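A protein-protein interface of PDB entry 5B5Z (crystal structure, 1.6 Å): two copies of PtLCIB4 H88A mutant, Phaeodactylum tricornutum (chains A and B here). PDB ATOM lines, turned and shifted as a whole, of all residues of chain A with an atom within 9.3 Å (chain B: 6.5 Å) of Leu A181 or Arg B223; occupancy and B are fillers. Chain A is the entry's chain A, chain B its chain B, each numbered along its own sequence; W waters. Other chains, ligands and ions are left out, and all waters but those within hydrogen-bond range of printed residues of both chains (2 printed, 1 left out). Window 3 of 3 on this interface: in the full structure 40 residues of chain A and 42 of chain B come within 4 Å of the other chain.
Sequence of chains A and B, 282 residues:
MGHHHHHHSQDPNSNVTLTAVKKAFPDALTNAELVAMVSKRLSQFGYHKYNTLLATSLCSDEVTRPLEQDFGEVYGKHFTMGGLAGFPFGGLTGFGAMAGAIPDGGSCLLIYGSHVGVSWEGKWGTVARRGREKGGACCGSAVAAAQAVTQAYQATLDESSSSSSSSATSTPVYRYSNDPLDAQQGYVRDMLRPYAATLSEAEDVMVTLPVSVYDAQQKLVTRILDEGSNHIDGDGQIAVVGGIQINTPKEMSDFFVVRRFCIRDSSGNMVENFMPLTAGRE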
ATOM      1  N   LEU A  84     -13.897  -6.335 -27.502  1.00  0.00           N
ATOM      2  CA  LEU A  84     -14.831  -5.968 -28.565  1.00  0.00           C
ATOM      3  C   LEU A  84     -14.139  -5.842 -29.927  1.00  0.00           C
ATOM      4  O   LEU A  84     -13.083  -5.235 -30.047  1.00  0.00           O
ATOM      5  CB  LEU A  84     -15.537  -4.659 -28.199  1.00  0.00           C
ATOM      6  CG  LEU A  84     -16.456  -4.763 -26.977  1.00  0.00           C
ATOM      7  CD1 LEU A  84     -17.025  -3.402 -26.669  1.00  0.00           C
ATOM      8  CD2 LEU A  84     -17.560  -5.791 -27.224  1.00  0.00           C
ATOM      9  N   PRO A 180     -14.487   3.480 -17.419  1.00  0.00           N
ATOM     10  CA  PRO A 180     -14.302   2.083 -17.823  1.00  0.00           C
ATOM     11  C   PRO A 180     -15.584   1.459 -18.314  1.00  0.00           C
ATOM     12  O   PRO A 180     -15.539   0.439 -19.030  1.00  0.00           O
ATOM     13  CB  PRO A 180     -13.833   1.396 -16.528  1.00  0.00           C
ATOM     14  CG  PRO A 180     -14.353   2.272 -15.415  1.00  0.00           C
ATOM     15  CD  PRO A 180     -14.804   3.604 -15.986  1.00  0.00           C
ATOM     16  N   LEU A 181     -16.709   2.075 -17.956  1.00  0.00           N
ATOM     17  CA  LEU A 181     -18.033   1.507 -18.173  1.00  0.00           C
ATOM     18  C   LEU A 181     -18.317   1.212 -19.632  1.00  0.00           C
ATOM     19  O   LEU A 181     -19.073   0.299 -19.928  1.00  0.00           O
ATOM     20  CB  LEU A 181     -19.104   2.449 -17.624  1.00  0.00           C
ATOM     21  CG  LEU A 181     -20.336   1.697 -17.139  1.00  0.00           C
ATOM     22  CD1 LEU A 181     -19.928   0.730 -16.048  1.00  0.00           C
ATOM     23  CD2 LEU A 181     -21.389   2.646 -16.604  1.00  0.00           C
ATOM     24  N   ASP A 182     -17.728   1.978 -20.545  1.00  0.00           N
ATOM     25  CA  ASP A 182     -17.861   1.643 -21.959  1.00  0.00           C
ATOM     26  C   ASP A 182     -16.624   2.046 -22.756  1.00  0.00           C
ATOM     27  O   ASP A 182     -16.720   2.452 -23.915  1.00  0.00           O
ATOM     28  CB  ASP A 182     -19.116   2.296 -22.545  1.00  0.00           C
ATOM     29  CG  ASP A 182     -19.681   1.510 -23.708  1.00  0.00           C
ATOM     30  OD1 ASP A 182     -19.407   0.298 -23.789  1.00  0.00           O
ATOM     31  OD2 ASP A 182     -20.406   2.101 -24.536  1.00  0.00           O
ATOM     32  N   ALA A 183     -15.454   1.888 -22.142  1.00  0.00           N
ATOM     33  CA  ALA A 183     -14.214   2.359 -22.750  1.00  0.00           C
ATOM     34  C   ALA A 183     -13.791   1.570 -23.994  1.00  0.00           C
ATOM     35  O   ALA A 183     -13.242   2.148 -24.937  1.00  0.00           O
ATOM     36  CB  ALA A 183     -13.093   2.347 -21.724  1.00  0.00           C
ATOM     37  N   GLN A 184     -14.030   0.261 -24.012  1.00  0.00           N
ATOM     38  CA  GLN A 184     -13.645  -0.526 -25.181  1.00  0.00           C
ATOM     39  C   GLN A 184     -14.316  -0.070 -26.467  1.00  0.00           C
ATOM     40  O   GLN A 184     -13.671   0.057 -27.508  1.00  0.00           O
ATOM     41  CB  GLN A 184     -13.942  -2.015 -24.951  1.00  0.00           C
ATOM     42  CG  GLN A 184     -12.674  -2.776 -24.663  1.00  0.00           C
ATOM     43  CD  GLN A 184     -12.850  -4.255 -24.390  1.00  0.00           C
ATOM     44  OE1 GLN A 184     -13.686  -4.940 -24.979  1.00  0.00           O
ATOM     45  NE2 GLN A 184     -12.024  -4.761 -23.490  1.00  0.00           N
ATOM     46  N   GLN A 185     -15.620   0.178 -26.419  1.00  0.00           N
ATOM     47  CA  GLN A 185     -16.302   0.551 -27.638  1.00  0.00           C
ATOM     48  C   GLN A 185     -15.793   1.916 -28.112  1.00  0.00           C
ATOM     49  O   GLN A 185     -15.744   2.170 -29.297  1.00  0.00           O
ATOM     50  CB  GLN A 185     -17.817   0.571 -27.449  1.00  0.00           C
ATOM     51  CG  GLN A 185     -18.601   0.841 -28.732  1.00  0.00           C
ATOM     52  CD  GLN A 185     -18.410  -0.223 -29.804  1.00  0.00           C
ATOM     53  OE1 GLN A 185     -17.850  -1.297 -29.548  1.00  0.00           O
ATOM     54  NE2 GLN A 185     -18.873   0.072 -31.010  1.00  0.00           N
ATOM     55  N   GLY A 186     -15.410   2.773 -27.174  1.00  0.00           N
ATOM     56  CA  GLY A 186     -14.838   4.062 -27.517  1.00  0.00           C
ATOM     57  C   GLY A 186     -13.516   3.869 -28.239  1.00  0.00           C
ATOM     58  O   GLY A 186     -13.218   4.571 -29.206  1.00  0.00           O
ATOM     59  N   PRO B  88     -15.105  -6.709 -15.959  1.00  0.00           N
ATOM     60  CA  PRO B  88     -15.983  -6.740 -17.147  1.00  0.00           C
ATOM     61  C   PRO B  88     -15.690  -5.599 -18.122  1.00  0.00           C
ATOM     62  O   PRO B  88     -16.500  -4.685 -18.319  1.00  0.00           O
ATOM     63  CB  PRO B  88     -17.395  -6.629 -16.549  1.00  0.00           C
ATOM     64  CG  PRO B  88     -17.196  -5.873 -15.259  1.00  0.00           C
ATOM     65  CD  PRO B  88     -15.855  -6.389 -14.730  1.00  0.00           C
ATOM     66  N   PHE B  89     -14.524  -5.676 -18.753  1.00  0.00           N
ATOM     67  CA  PHE B  89     -14.065  -4.622 -19.642  1.00  0.00           C
ATOM     68  C   PHE B  89     -14.913  -4.490 -20.909  1.00  0.00           C
ATOM     69  O   PHE B  89     -14.855  -3.455 -21.560  1.00  0.00           O
ATOM     70  CB  PHE B  89     -12.590  -4.846 -20.003  1.00  0.00           C
ATOM     71  CG  PHE B  89     -11.654  -4.509 -18.890  1.00  0.00           C
ATOM     72  CD1 PHE B  89     -11.519  -3.197 -18.464  1.00  0.00           C
ATOM     73  CD2 PHE B  89     -10.921  -5.496 -18.250  1.00  0.00           C
ATOM     74  CE1 PHE B  89     -10.656  -2.869 -17.437  1.00  0.00           C
ATOM     75  CE2 PHE B  89     -10.063  -5.174 -17.210  1.00  0.00           C
ATOM     76  CZ  PHE B  89      -9.929  -3.866 -16.802  1.00  0.00           C
ATOM     77  N   GLY B  90     -15.701  -5.512 -21.241  1.00  0.00           N
ATOM     78  CA  GLY B  90     -16.643  -5.407 -22.351  1.00  0.00           C
ATOM     79  C   GLY B  90     -17.609  -4.248 -22.136  1.00  0.00           C
ATOM     80  O   GLY B  90     -18.107  -3.619 -23.085  1.00  0.00           O
ATOM     81  N   GLY B  91     -17.869  -3.954 -20.871  1.00  0.00           N
ATOM     82  CA  GLY B  91     -18.661  -2.787 -20.514  1.00  0.00           C
ATOM     83  C   GLY B  91     -20.085  -2.826 -21.043  1.00  0.00           C
ATOM     84  O   GLY B  91     -20.631  -3.887 -21.323  1.00  0.00           O
ATOM     85  N   LEU B  92     -20.682  -1.645 -21.180  1.00  0.00           N
ATOM     86  CA  LEU B  92     -22.077  -1.542 -21.569  1.00  0.00           C
ATOM     87  C   LEU B  92     -22.332  -2.122 -22.944  1.00  0.00           C
ATOM     88  O   LEU B  92     -23.337  -2.785 -23.173  1.00  0.00           O
ATOM     89  CB  LEU B  92     -22.521  -0.078 -21.547  1.00  0.00           C
ATOM     90  CG  LEU B  92     -22.474   0.603 -20.186  1.00  0.00           C
ATOM     91  CD1 LEU B  92     -23.038   2.021 -20.301  1.00  0.00           C
ATOM     92  CD2 LEU B  92     -23.255  -0.198 -19.169  1.00  0.00           C
ATOM     93  N   THR B  93     -21.426  -1.841 -23.871  1.00  0.00           N
ATOM     94  CA  THR B  93     -21.603  -2.301 -25.235  1.00  0.00           C
ATOM     95  C   THR B  93     -21.488  -3.819 -25.284  1.00  0.00           C
ATOM     96  O   THR B  93     -22.241  -4.486 -25.986  1.00  0.00           O
ATOM     97  CB  THR B  93     -20.578  -1.640 -26.197  1.00  0.00           C
ATOM     98  OG1 THR B  93     -20.892  -0.243 -26.314  1.00  0.00           O
ATOM     99  CG2 THR B  93     -20.637  -2.276 -27.581  1.00  0.00           C
ATOM    100  N   GLN B 218     -17.704  -6.827  -8.265  1.00  0.00           N
ATOM    101  CA  GLN B 218     -19.120  -6.963  -7.969  1.00  0.00           C
ATOM    102  C   GLN B 218     -19.797  -5.609  -8.135  1.00  0.00           C
ATOM    103  O   GLN B 218     -20.899  -5.523  -8.663  1.00  0.00           O
ATOM    104  CB  GLN B 218     -19.325  -7.531  -6.563  1.00  0.00           C
ATOM    105  CG  GLN B 218     -20.750  -7.458  -6.045  1.00  0.00           C
ATOM    106  CD  GLN B 218     -21.013  -6.154  -5.303  1.00  0.00           C
ATOM    107  OE1 GLN B 218     -20.286  -5.790  -4.375  1.00  0.00           O
ATOM    108  NE2 GLN B 218     -22.019  -5.432  -5.738  1.00  0.00           N
ATOM    109  N   LYS B 219     -19.113  -4.551  -7.706  1.00  0.00           N
ATOM    110  CA  LYS B 219     -19.652  -3.199  -7.854  1.00  0.00           C
ATOM    111  C   LYS B 219     -19.812  -2.798  -9.325  1.00  0.00           C
ATOM    112  O   LYS B 219     -20.839  -2.220  -9.715  1.00  0.00           O
ATOM    113  CB  LYS B 219     -18.759  -2.187  -7.131  1.00  0.00           C
ATOM    114  CG  LYS B 219     -18.675  -2.383  -5.627  1.00  0.00           C
ATOM    115  CD  LYS B 219     -18.005  -1.175  -4.975  1.00  0.00           C
ATOM    116  CE  LYS B 219     -17.496  -1.467  -3.572  1.00  0.00           C
ATOM    117  NZ  LYS B 219     -18.526  -2.108  -2.718  1.00  0.00           N
ATOM    118  N   LEU B 220     -18.796  -3.089 -10.132  1.00  0.00           N
ATOM    119  CA  LEU B 220     -18.830  -2.726 -11.542  1.00  0.00           C
ATOM    120  C   LEU B 220     -19.879  -3.540 -12.292  1.00  0.00           C
ATOM    121  O   LEU B 220     -20.628  -2.990 -13.109  1.00  0.00           O
ATOM    122  CB  LEU B 220     -17.441  -2.901 -12.174  1.00  0.00           C
ATOM    123  CG  LEU B 220     -17.353  -2.521 -13.657  1.00  0.00           C
ATOM    124  CD1 LEU B 220     -17.790  -1.079 -13.893  1.00  0.00           C
ATOM    125  CD2 LEU B 220     -15.937  -2.719 -14.170  1.00  0.00           C
ATOM    126  N   VAL B 221     -19.942  -4.845 -12.013  1.00  0.00           N
ATOM    127  CA  VAL B 221     -20.972  -5.679 -12.636  1.00  0.00           C
ATOM    128  C   VAL B 221     -22.376  -5.157 -12.295  1.00  0.00           C
ATOM    129  O   VAL B 221     -23.234  -5.033 -13.177  1.00  0.00           O
ATOM    130  CB  VAL B 221     -20.843  -7.165 -12.208  1.00  0.00           C
ATOM    131  CG1 VAL B 221     -22.062  -7.959 -12.689  1.00  0.00           C
ATOM    132  CG2 VAL B 221     -19.564  -7.778 -12.764  1.00  0.00           C
ATOM    133  N   THR B 222     -22.598  -4.834 -11.025  1.00  0.00           N
ATOM    134  CA  THR B 222     -23.895  -4.308 -10.612  1.00  0.00           C
ATOM    135  C   THR B 222     -24.230  -3.029 -11.377  1.00  0.00           C
ATOM    136  O   THR B 222     -25.345  -2.876 -11.869  1.00  0.00           O
ATOM    137  CB  THR B 222     -23.934  -4.046  -9.104  1.00  0.00           C
ATOM    138  OG1 THR B 222     -23.837  -5.298  -8.414  1.00  0.00           O
ATOM    139  CG2 THR B 222     -25.237  -3.344  -8.697  1.00  0.00           C
ATOM    140  N   ARG B 223     -23.254  -2.135 -11.523  1.00  0.00           N
ATOM    141  CA  ARG B 223     -23.459  -0.912 -12.304  1.00  0.00           C
ATOM    142  C   ARG B 223     -23.813  -1.183 -13.769  1.00  0.00           C
ATOM    143  O   ARG B 223     -24.718  -0.561 -14.323  1.00  0.00           O
ATOM    144  CB  ARG B 223     -22.215  -0.018 -12.247  1.00  0.00           C
ATOM    145  CG  ARG B 223     -22.359   1.283 -13.046  1.00  0.00           C
ATOM    146  CD  ARG B 223     -21.172   2.204 -12.834  1.00  0.00           C
ATOM    147  NE  ARG B 223     -21.129   2.735 -11.470  1.00  0.00           N
ATOM    148  CZ  ARG B 223     -20.070   3.344 -10.942  1.00  0.00           C
ATOM    149  NH1 ARG B 223     -18.965   3.493 -11.662  1.00  0.00           N
ATOM    150  NH2 ARG B 223     -20.114   3.812  -9.702  1.00  0.00           N
ATOM    151  N   ILE B 224     -23.090  -2.102 -14.404  1.00  0.00           N
ATOM    152  CA  ILE B 224     -23.367  -2.446 -15.794  1.00  0.00           C
ATOM    153  C   ILE B 224     -24.786  -3.012 -15.947  1.00  0.00           C
ATOM    154  O   ILE B 224     -25.529  -2.622 -16.847  1.00  0.00           O
ATOM    155  CB  ILE B 224     -22.333  -3.469 -16.320  1.00  0.00           C
ATOM    156  CG1 ILE B 224     -20.964  -2.802 -16.483  1.00  0.00           C
ATOM    157  CG2 ILE B 224     -22.786  -4.083 -17.645  1.00  0.00           C
ATOM    158  CD1 ILE B 224     -19.828  -3.795 -16.728  1.00  0.00           C
ATOM    159  N   LEU B 225     -25.163  -3.919 -15.052  1.00  0.00           N
ATOM    160  CA  LEU B 225     -26.493  -4.524 -15.115  1.00  0.00           C
ATOM    161  C   LEU B 225     -27.591  -3.491 -14.875  1.00  0.00           C
ATOM    162  O   LEU B 225     -28.654  -3.561 -15.488  1.00  0.00           O
ATOM    163  CB  LEU B 225     -26.632  -5.656 -14.095  1.00  0.00           C
ATOM    164  CG  LEU B 225     -25.705  -6.860 -14.233  1.00  0.00           C
ATOM    165  CD1 LEU B 225     -26.038  -7.898 -13.185  1.00  0.00           C
ATOM    166  CD2 LEU B 225     -25.827  -7.433 -15.600  1.00  0.00           C
ATOM    167  N   ASP B 226     -27.335  -2.542 -13.978  1.00  0.00           N
ATOM    168  CA  ASP B 226     -28.297  -1.471 -13.708  1.00  0.00           C
ATOM    169  C   ASP B 226     -28.474  -0.589 -14.947  1.00  0.00           C
ATOM    170  O   ASP B 226     -29.597  -0.189 -15.284  1.00  0.00           O
ATOM    171  CB  ASP B 226     -27.854  -0.627 -12.501  1.00  0.00           C
ATOM    172  CG  ASP B 226     -28.018  -1.364 -11.172  1.00  0.00           C
ATOM    173  OD1 ASP B 226     -28.678  -2.421 -11.144  1.00  0.00           O
ATOM    174  OD2 ASP B 226     -27.493  -0.880 -10.141  1.00  0.00           O
ATOM    175  N   GLU B 227     -27.375  -0.308 -15.640  1.00  0.00           N
ATOM    176  CA  GLU B 227     -27.420   0.536 -16.840  1.00  0.00           C
ATOM    177  C   GLU B 227     -28.038  -0.145 -18.050  1.00  0.00           C
ATOM    178  O   GLU B 227     -28.848   0.452 -18.758  1.00  0.00           O
ATOM    179  CB  GLU B 227     -26.016   0.994 -17.221  1.00  0.00           C
ATOM    180  CG  GLU B 227     -25.359   1.856 -16.197  1.00  0.00           C
ATOM    181  CD  GLU B 227     -25.797   3.295 -16.293  1.00  0.00           C
ATOM    182  OE1 GLU B 227     -26.380   3.682 -17.334  1.00  0.00           O
ATOM    183  OE2 GLU B 227     -25.535   4.038 -15.335  1.00  0.00           O
ATOM    184  N   GLY B 228     -27.633  -1.386 -18.300  1.00  0.00           N
ATOM    185  CA  GLY B 228     -28.049  -2.095 -19.499  1.00  0.00           C
ATOM    186  C   GLY B 228     -29.320  -2.887 -19.285  1.00  0.00           C
ATOM    187  O   GLY B 228     -29.599  -3.852 -20.009  1.00  0.00           O
HETATM  188  O   HOH W   1     -16.313  -1.798 -17.911  1.00  0.00           O
HETATM  189  O   HOH W   2     -17.094  -1.078 -24.002  1.00  0.00           O
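No position is printed for both chains. Of the 12 pairs that touch across the chains among the printed residues, none has its exchanged pair printed and touching as well.
Of chain B, only Gly B91 (3.2 Å), Leu B92 (2.8 Å), Leu B220 (3.5 Å), Arg B223 (3.7 Å) and Ile B224 (3.7 Å) come within 4 Å of Leu A181. Of the printed residues of chain B, Asp A182 touches Leu B92 (3.5 Å) and Thr B93 (2.9 Å). Of the printed residues of chain B, Gln A184 touches Phe B89 (3.5 Å) and Gly B90 (3.98 Å). Printed residues of chain B within 4 Å of Gln A185: Thr B93 (3.4 Å). Gly A186 touches none of the printed residues of chain B. Of the printed residues of chain A, Phe B89 touches Gln A184. Gln B218 touches none of the printed residues of chain A. Of the printed residues of chain A, Leu B220 touches Leu A181. No residue of chain A comes within 4 Å of Thr B222. Arg B223 touches one residue of chain A. Ile B224 touches just one residue of chain A: Leu A181. The nearest residue of chain B that does not touch Leu A181 is Glu B227 (4.1 Å). The nearest printed residue of chain A that does not touch Gly B90 is Asp A182 (4.2 Å).
O of Leu A181 lies within hydrogen-bond range of N of Leu B92 (2.8 Å). N of Leu B92 sits at hydrogen-bond distance from OD1 of Asp A182 (3.5 Å). The side-chain carboxylate (OD1) of Asp A182 lies within hydrogen-bond range of the backbone NH (N) of Thr B93, 2.9 Å away.
Water W1 bridges O of Pro A180 and O of Pro B88. Water W2 lies within hydrogen-bond range of the side-chain carboxylate of Asp A182 (2.7 Å), the backbone carbonyl oxygen of Gly B90 (2.9 Å), the backbone NH of Gln A185 (3.1 Å) and the backbone NH of Gln A184 (3.3 Å).
Leu A84 touches Gly B90 (CD1 to O, 3.8 Å). Leu A84 touches Thr B93. Gly B91 touches Leu A181. Leu A181 touches Leu B220. Arg B223 touches Leu A181 (CD to CD1, 3.7 Å). Ile B224 touches Leu A181. CB of Phe B89 touches NE2 of Gln A184, 3.5 Å away. OE1 of Gln A184 touches CA of Gly B90, at 3.98 Å. OG1 of Thr B93 touches CB of Gln A185, at 3.4 Å.
Of the 17 printed residues of chain B, 8 touch a printed residue of chain A. Hydrophobic or aromatic side chains of chain B within 4 Å of the printed part of chain A: Phe B89, Leu B92, Leu B220 and Ile B224. Along chain B the printed residues that touch a printed residue of chain A span positions 89 to 224. Of the 8 printed residues of chain A, 5 touch a printed residue of chain B. Hydrophobic or aromatic side chains of chain A within 4 Å of the printed part of chain B: Leu A84 and Leu A181. Along chain A the printed residues that touch a printed residue of chain B span positions 84 to 185. Among the printed residues, 12 pairs touch across the chains. Among the printed residues, no Asp or Glu carboxylate lies within 4 Å of a Lys or Arg side-chain nitrogen of the other chain.
N of Leu A84 is in hydrogen-bond range of OE1 of Gln A184.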
